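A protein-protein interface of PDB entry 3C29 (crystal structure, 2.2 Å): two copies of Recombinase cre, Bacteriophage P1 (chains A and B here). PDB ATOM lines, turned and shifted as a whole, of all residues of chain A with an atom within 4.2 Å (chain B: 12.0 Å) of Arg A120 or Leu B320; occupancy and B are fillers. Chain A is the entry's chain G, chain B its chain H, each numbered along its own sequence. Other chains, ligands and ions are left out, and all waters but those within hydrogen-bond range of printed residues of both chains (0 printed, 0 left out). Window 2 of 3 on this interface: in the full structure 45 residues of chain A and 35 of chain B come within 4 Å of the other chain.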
ATOM      1  N   GLU A 119      26.582  24.569  -5.303  1.00  0.00           N
ATOM      2  CA  GLU A 119      25.969  23.266  -5.061  1.00  0.00           C
ATOM      3  C   GLU A 119      27.041  22.178  -4.922  1.00  0.00           C
ATOM      4  O   GLU A 119      28.252  22.469  -5.006  1.00  0.00           O
ATOM      5  CB  GLU A 119      24.985  22.938  -6.209  1.00  0.00           C
ATOM      6  CG  GLU A 119      23.894  24.022  -6.396  1.00  0.00           C
ATOM      7  CD  GLU A 119      22.909  23.715  -7.532  1.00  0.00           C
ATOM      8  OE1 GLU A 119      23.349  23.489  -8.690  1.00  0.00           O
ATOM      9  OE2 GLU A 119      21.687  23.703  -7.256  1.00  0.00           O
ATOM     10  N   ARG A 120      26.595  20.944  -4.696  1.00  0.00           N
ATOM     11  CA  ARG A 120      27.484  19.774  -4.585  1.00  0.00           C
ATOM     12  C   ARG A 120      28.357  19.619  -5.841  1.00  0.00           C
ATOM     13  O   ARG A 120      29.565  19.414  -5.738  1.00  0.00           O
ATOM     14  CB  ARG A 120      26.659  18.495  -4.328  1.00  0.00           C
ATOM     15  CG  ARG A 120      27.464  17.177  -4.341  1.00  0.00           C
ATOM     16  CD  ARG A 120      28.526  17.130  -3.229  1.00  0.00           C
ATOM     17  NE  ARG A 120      29.211  15.826  -3.167  1.00  0.00           N
ATOM     18  CZ  ARG A 120      28.723  14.737  -2.565  1.00  0.00           C
ATOM     19  NH1 ARG A 120      27.542  14.758  -1.946  1.00  0.00           N
ATOM     20  NH2 ARG A 120      29.420  13.616  -2.588  1.00  0.00           N
ATOM     21  N   THR A 121      27.746  19.752  -7.020  1.00  0.00           N
ATOM     22  CA  THR A 121      28.499  19.676  -8.272  1.00  0.00           C
ATOM     23  C   THR A 121      29.636  20.697  -8.315  1.00  0.00           C
ATOM     24  O   THR A 121      30.728  20.363  -8.771  1.00  0.00           O
ATOM     25  CB  THR A 121      27.606  19.805  -9.538  1.00  0.00           C
ATOM     26  OG1 THR A 121      26.862  21.027  -9.483  1.00  0.00           O
ATOM     27  CG2 THR A 121      26.642  18.607  -9.645  1.00  0.00           C
ATOM     28  N   ASP A 122      29.385  21.914  -7.819  1.00  0.00           N
ATOM     29  CA  ASP A 122      30.407  22.975  -7.750  1.00  0.00           C
ATOM     30  C   ASP A 122      31.477  22.707  -6.716  1.00  0.00           C
ATOM     31  O   ASP A 122      32.659  22.967  -6.950  1.00  0.00           O
ATOM     32  CB  ASP A 122      29.763  24.333  -7.458  1.00  0.00           C
ATOM     33  CG  ASP A 122      28.617  24.638  -8.398  1.00  0.00           C
ATOM     34  OD1 ASP A 122      28.884  24.848  -9.600  1.00  0.00           O
ATOM     35  OD2 ASP A 122      27.456  24.665  -7.935  1.00  0.00           O
ATOM     36  N   PHE A 123      31.045  22.222  -5.558  1.00  0.00           N
ATOM     37  CA  PHE A 123      31.946  21.841  -4.480  1.00  0.00           C
ATOM     38  C   PHE A 123      32.899  20.681  -4.855  1.00  0.00           C
ATOM     39  O   PHE A 123      34.082  20.742  -4.537  1.00  0.00           O
ATOM     40  CB  PHE A 123      31.142  21.487  -3.223  1.00  0.00           C
ATOM     41  CG  PHE A 123      31.998  21.127  -2.034  1.00  0.00           C
ATOM     42  CD1 PHE A 123      33.054  21.946  -1.643  1.00  0.00           C
ATOM     43  CD2 PHE A 123      31.716  19.995  -1.289  1.00  0.00           C
ATOM     44  CE1 PHE A 123      33.838  21.626  -0.551  1.00  0.00           C
ATOM     45  CE2 PHE A 123      32.495  19.657  -0.190  1.00  0.00           C
ATOM     46  CZ  PHE A 123      33.557  20.478   0.183  1.00  0.00           C
ATOM     47  N   ASP A 124      32.362  19.642  -5.497  1.00  0.00           N
ATOM     48  CA  ASP A 124      33.167  18.525  -6.023  1.00  0.00           C
ATOM     49  C   ASP A 124      34.186  19.030  -7.035  1.00  0.00           C
ATOM     50  O   ASP A 124      35.362  18.697  -6.954  1.00  0.00           O
ATOM     51  CB  ASP A 124      32.279  17.460  -6.681  1.00  0.00           C
ATOM     52  CG  ASP A 124      31.536  16.584  -5.667  1.00  0.00           C
ATOM     53  OD1 ASP A 124      31.935  16.516  -4.489  1.00  0.00           O
ATOM     54  OD2 ASP A 124      30.534  15.945  -6.060  1.00  0.00           O
ATOM     55  N   TYR A 149      28.987  25.048   2.919  1.00  0.00           N
ATOM     56  CA  TYR A 149      28.076  24.125   2.279  1.00  0.00           C
ATOM     57  C   TYR A 149      27.540  23.101   3.283  1.00  0.00           C
ATOM     58  O   TYR A 149      26.330  22.821   3.317  1.00  0.00           O
ATOM     59  CB  TYR A 149      28.726  23.424   1.061  1.00  0.00           C
ATOM     60  CG  TYR A 149      27.780  22.430   0.382  1.00  0.00           C
ATOM     61  CD1 TYR A 149      26.769  22.872  -0.501  1.00  0.00           C
ATOM     62  CD2 TYR A 149      27.877  21.060   0.642  1.00  0.00           C
ATOM     63  CE1 TYR A 149      25.885  21.959  -1.110  1.00  0.00           C
ATOM     64  CE2 TYR A 149      27.001  20.141   0.041  1.00  0.00           C
ATOM     65  CZ  TYR A 149      26.011  20.601  -0.823  1.00  0.00           C
ATOM     66  OH  TYR A 149      25.153  19.688  -1.385  1.00  0.00           O
ATOM     67  N   ASN A 150      28.437  22.544   4.100  1.00  0.00           N
ATOM     68  CA  ASN A 150      28.058  21.516   5.068  1.00  0.00           C
ATOM     69  C   ASN A 150      27.067  22.051   6.109  1.00  0.00           C
ATOM     70  O   ASN A 150      26.108  21.381   6.429  1.00  0.00           O
ATOM     71  CB  ASN A 150      29.304  20.955   5.779  1.00  0.00           C
ATOM     72  CG  ASN A 150      29.092  19.566   6.388  1.00  0.00           C
ATOM     73  OD1 ASN A 150      30.030  18.773   6.434  1.00  0.00           O
ATOM     74  ND2 ASN A 150      27.882  19.271   6.877  1.00  0.00           N
ATOM     75  N   SER A 195      30.703  16.435   7.791  1.00  0.00           N
ATOM     76  CA  SER A 195      30.883  15.101   7.225  1.00  0.00           C
ATOM     77  C   SER A 195      32.349  14.694   7.393  1.00  0.00           C
ATOM     78  O   SER A 195      33.208  15.524   7.720  1.00  0.00           O
ATOM     79  CB  SER A 195      30.505  15.059   5.747  1.00  0.00           C
ATOM     80  OG  SER A 195      31.338  15.935   5.007  1.00  0.00           O
ATOM     81  N   ASP A 279      20.189  20.985  -3.058  1.00  0.00           N
ATOM     82  CA  ASP A 279      20.653  19.594  -3.053  1.00  0.00           C
ATOM     83  C   ASP A 279      19.820  18.698  -2.155  1.00  0.00           C
ATOM     84  O   ASP A 279      19.532  17.542  -2.515  1.00  0.00           O
ATOM     85  CB  ASP A 279      22.146  19.510  -2.695  1.00  0.00           C
ATOM     86  CG  ASP A 279      23.026  20.037  -3.825  1.00  0.00           C
ATOM     87  OD1 ASP A 279      22.544  20.011  -4.986  1.00  0.00           O
ATOM     88  OD2 ASP A 279      24.170  20.495  -3.562  1.00  0.00           O
ATOM     89  N   SER B 311      22.547  16.562  14.394  1.00  0.00           N
ATOM     90  CA  SER B 311      23.242  17.056  13.218  1.00  0.00           C
ATOM     91  C   SER B 311      24.063  15.946  12.537  1.00  0.00           C
ATOM     92  O   SER B 311      24.087  15.832  11.303  1.00  0.00           O
ATOM     93  CB  SER B 311      24.131  18.246  13.592  1.00  0.00           C
ATOM     94  OG  SER B 311      24.549  18.897  12.410  1.00  0.00           O
ATOM     95  N   GLU B 312      24.721  15.134  13.351  1.00  0.00           N
ATOM     96  CA  GLU B 312      25.572  14.059  12.854  1.00  0.00           C
ATOM     97  C   GLU B 312      24.850  13.035  11.972  1.00  0.00           C
ATOM     98  O   GLU B 312      25.428  12.533  11.016  1.00  0.00           O
ATOM     99  CB  GLU B 312      26.338  13.382  13.991  1.00  0.00           C
ATOM    100  CG  GLU B 312      27.460  12.513  13.468  1.00  0.00           C
ATOM    101  CD  GLU B 312      28.381  11.965  14.550  1.00  0.00           C
ATOM    102  OE1 GLU B 312      28.060  12.102  15.762  1.00  0.00           O
ATOM    103  OE2 GLU B 312      29.432  11.389  14.169  1.00  0.00           O
ATOM    104  N   THR B 313      23.592  12.752  12.276  1.00  0.00           N
ATOM    105  CA  THR B 313      22.764  11.869  11.446  1.00  0.00           C
ATOM    106  C   THR B 313      21.791  12.673  10.583  1.00  0.00           C
ATOM    107  O   THR B 313      20.838  12.124  10.030  1.00  0.00           O
ATOM    108  CB  THR B 313      22.013  10.812  12.309  1.00  0.00           C
ATOM    109  OG1 THR B 313      21.114  11.461  13.237  1.00  0.00           O
ATOM    110  CG2 THR B 313      23.042   9.951  13.082  1.00  0.00           C
ATOM    111  N   GLY B 314      22.063  13.978  10.467  1.00  0.00           N
ATOM    112  CA  GLY B 314      21.181  14.914   9.782  1.00  0.00           C
ATOM    113  C   GLY B 314      21.356  14.826   8.288  1.00  0.00           C
ATOM    114  O   GLY B 314      22.213  14.092   7.785  1.00  0.00           O
ATOM    115  N   ALA B 315      20.557  15.605   7.579  1.00  0.00           N
ATOM    116  CA  ALA B 315      20.457  15.499   6.135  1.00  0.00           C
ATOM    117  C   ALA B 315      21.775  15.843   5.401  1.00  0.00           C
ATOM    118  O   ALA B 315      22.178  15.134   4.488  1.00  0.00           O
ATOM    119  CB  ALA B 315      19.264  16.350   5.622  1.00  0.00           C
ATOM    120  N   MET B 316      22.453  16.906   5.820  1.00  0.00           N
ATOM    121  CA  MET B 316      23.677  17.327   5.136  1.00  0.00           C
ATOM    122  C   MET B 316      24.832  16.333   5.255  1.00  0.00           C
ATOM    123  O   MET B 316      25.511  16.054   4.259  1.00  0.00           O
ATOM    124  CB  MET B 316      24.121  18.724   5.579  1.00  0.00           C
ATOM    125  CG  MET B 316      23.237  19.867   5.061  1.00  0.00           C
ATOM    126  SD  MET B 316      22.881  19.842   3.292  1.00  0.00           S
ATOM    127  CE  MET B 316      24.526  19.923   2.570  1.00  0.00           C
ATOM    128  N   VAL B 317      25.061  15.806   6.455  1.00  0.00           N
ATOM    129  CA  VAL B 317      26.100  14.777   6.632  1.00  0.00           C
ATOM    130  C   VAL B 317      25.803  13.531   5.767  1.00  0.00           C
ATOM    131  O   VAL B 317      26.690  13.039   5.070  1.00  0.00           O
ATOM    132  CB  VAL B 317      26.306  14.400   8.108  1.00  0.00           C
ATOM    133  CG1 VAL B 317      27.149  13.131   8.231  1.00  0.00           C
ATOM    134  CG2 VAL B 317      26.960  15.551   8.848  1.00  0.00           C
ATOM    135  N   ARG B 318      24.552  13.061   5.803  1.00  0.00           N
ATOM    136  CA  ARG B 318      24.104  11.934   4.973  1.00  0.00           C
ATOM    137  C   ARG B 318      24.285  12.204   3.473  1.00  0.00           C
ATOM    138  O   ARG B 318      24.766  11.330   2.738  1.00  0.00           O
ATOM    139  CB  ARG B 318      22.645  11.563   5.287  1.00  0.00           C
ATOM    140  CG  ARG B 318      22.421  11.105   6.745  1.00  0.00           C
ATOM    141  CD  ARG B 318      21.078  10.379   6.982  1.00  0.00           C
ATOM    142  NE  ARG B 318      19.955  10.936   6.200  1.00  0.00           N
ATOM    143  CZ  ARG B 318      19.013  11.760   6.668  1.00  0.00           C
ATOM    144  NH1 ARG B 318      19.006  12.157   7.942  1.00  0.00           N
ATOM    145  NH2 ARG B 318      18.061  12.193   5.846  1.00  0.00           N
ATOM    146  N   LEU B 319      23.941  13.423   3.036  1.00  0.00           N
ATOM    147  CA  LEU B 319      24.096  13.813   1.631  1.00  0.00           C
ATOM    148  C   LEU B 319      25.549  13.792   1.211  1.00  0.00           C
ATOM    149  O   LEU B 319      25.883  13.323   0.120  1.00  0.00           O
ATOM    150  CB  LEU B 319      23.534  15.218   1.362  1.00  0.00           C
ATOM    151  CG  LEU B 319      22.198  15.408   0.651  1.00  0.00           C
ATOM    152  CD1 LEU B 319      21.975  16.858   0.405  1.00  0.00           C
ATOM    153  CD2 LEU B 319      22.186  14.673  -0.675  1.00  0.00           C
ATOM    154  N   LEU B 320      26.410  14.324   2.078  1.00  0.00           N
ATOM    155  CA  LEU B 320      27.817  14.445   1.735  1.00  0.00           C
ATOM    156  C   LEU B 320      28.523  13.094   1.727  1.00  0.00           C
ATOM    157  O   LEU B 320      29.374  12.855   0.888  1.00  0.00           O
ATOM    158  CB  LEU B 320      28.530  15.458   2.635  1.00  0.00           C
ATOM    159  CG  LEU B 320      28.339  16.917   2.199  1.00  0.00           C
ATOM    160  CD1 LEU B 320      28.512  17.859   3.371  1.00  0.00           C
ATOM    161  CD2 LEU B 320      29.284  17.301   1.053  1.00  0.00           C
ATOM    162  N   GLU B 321      28.128  12.206   2.630  1.00  0.00           N
ATOM    163  CA  GLU B 321      28.810  10.927   2.809  1.00  0.00           C
ATOM    164  C   GLU B 321      28.276   9.772   1.940  1.00  0.00           C
ATOM    165  O   GLU B 321      28.867   8.689   1.921  1.00  0.00           O
ATOM    166  CB  GLU B 321      28.791  10.540   4.291  1.00  0.00           C
ATOM    167  CG  GLU B 321      29.686  11.446   5.130  1.00  0.00           C
ATOM    168  CD  GLU B 321      29.689  11.119   6.604  1.00  0.00           C
ATOM    169  OE1 GLU B 321      30.340  11.870   7.360  1.00  0.00           O
ATOM    170  OE2 GLU B 321      29.055  10.123   7.016  1.00  0.00           O
ATOM    171  N   ASP B 322      27.173   9.998   1.231  1.00  0.00           N
ATOM    172  CA  ASP B 322      26.522   8.925   0.471  1.00  0.00           C
ATOM    173  C   ASP B 322      25.557   9.476  -0.580  1.00  0.00           C
ATOM    174  O   ASP B 322      25.866  10.458  -1.265  1.00  0.00           O
ATOM    175  CB  ASP B 322      25.798   7.928   1.418  1.00  0.00           C
ATOM    176  CG  ASP B 322      26.656   6.685   1.768  1.00  0.00           C
ATOM    177  OD1 ASP B 322      26.841   6.406   2.986  1.00  0.00           O
ATOM    178  OD2 ASP B 322      27.131   5.986   0.829  1.00  0.00           O
ATOM    179  OXT ASP B 322      24.452   8.959  -0.785  1.00  0.00           O
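The backbone carbonyl oxygen (O) of Leu B319 sits at hydrogen-bond distance from the guanidinium group (NH1) of Arg A120, 3.0 Å away.
The guanidinium group (NE) of Arg A120 lies within salt-bridge range of the side-chain carboxylate (OD1) of Asp A124.
N of Arg A120 lies within hydrogen-bond range of OD2 of Asp A279 (2.7 Å).
The side-chain hydroxyl (OH) of Tyr A149 sits at hydrogen-bond distance from the side-chain carboxylate (OD2) of Asp A279 (2.5 Å).
The backbone NH (N) of Ser A195 is in hydrogen-bond range of the side-chain amide oxygen (OD1) of Asn A150, at 2.8 Å.
Among the printed residues, pairs that only touch across the chains: Arg A120 with Leu B320 (3.6 Å), Tyr A149 with Met B316 (3.5 Å), Tyr A149 with Leu B320 (3.8 Å), Asn A150 with Met B316 (3.4 Å), Asn A150 with Leu B320 (3.5 Å), Ser A195 with Val B317 (3.99 Å), Ser A195 with Leu B320 (3.7 Å), Ser A195 with Glu B321 (3.3 Å) and Asp A279 with Leu B319 (3.8 Å).
Arg A120 touches just these residues of chain B: Leu B319 (3.0 Å) and Leu B320 (3.6 Å).
Leu B320 touches just these residues of chain A: Arg A120, Tyr A149, Asn A150 and Ser A195.
Glu A119 touches none of the printed residues of chain B.
No residue of chain B comes within 4 Å of Thr A121.
Asp A122 touches none of the printed residues of chain B.
No residue of chain B comes within 4 Å of Phe A123.
Of chain B, only Met B316 (3.5 Å) and Leu B320 (3.8 Å) come within 4 Å of Tyr A149.
Asn A150 touches just these residues of chain B: Met B316 (3.4 Å) and Leu B320 (3.5 Å).
Asp A279 touches one residue of chain B.
Of the printed residues of chain A, Val B317 touches Ser A195.
Printed residues of chain B within 4 Å of Ser A195: Val B317 (3.99 Å), Leu B320 (3.7 Å) and Glu B321 (3.3 Å).
Of the printed residues of chain A, Leu B319 touches Arg A120 (3.0 Å) and Asp A279 (3.8 Å).
Of the printed residues of chain A, Glu B321 touches Ser A195 (3.3 Å).
The nearest residue of chain B that does not touch Arg A120 is Asp B322 (4.7 Å).
The nearest printed residue of chain A that does not touch Leu B320 is Phe A123 (4.2 Å).
Of the 10 printed residues of chain A, 5 touch a printed residue of chain B.
Hydrophobic or aromatic side chains of chain A that line the printed part of chain B: Tyr A149.
Along chain A the printed residues that touch a printed residue of chain B span positions 120 to 279.
No position is printed for both chains.
Of the 10 pairs that touch across the chains among the printed residues, none has its exchanged pair printed and touching as well.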
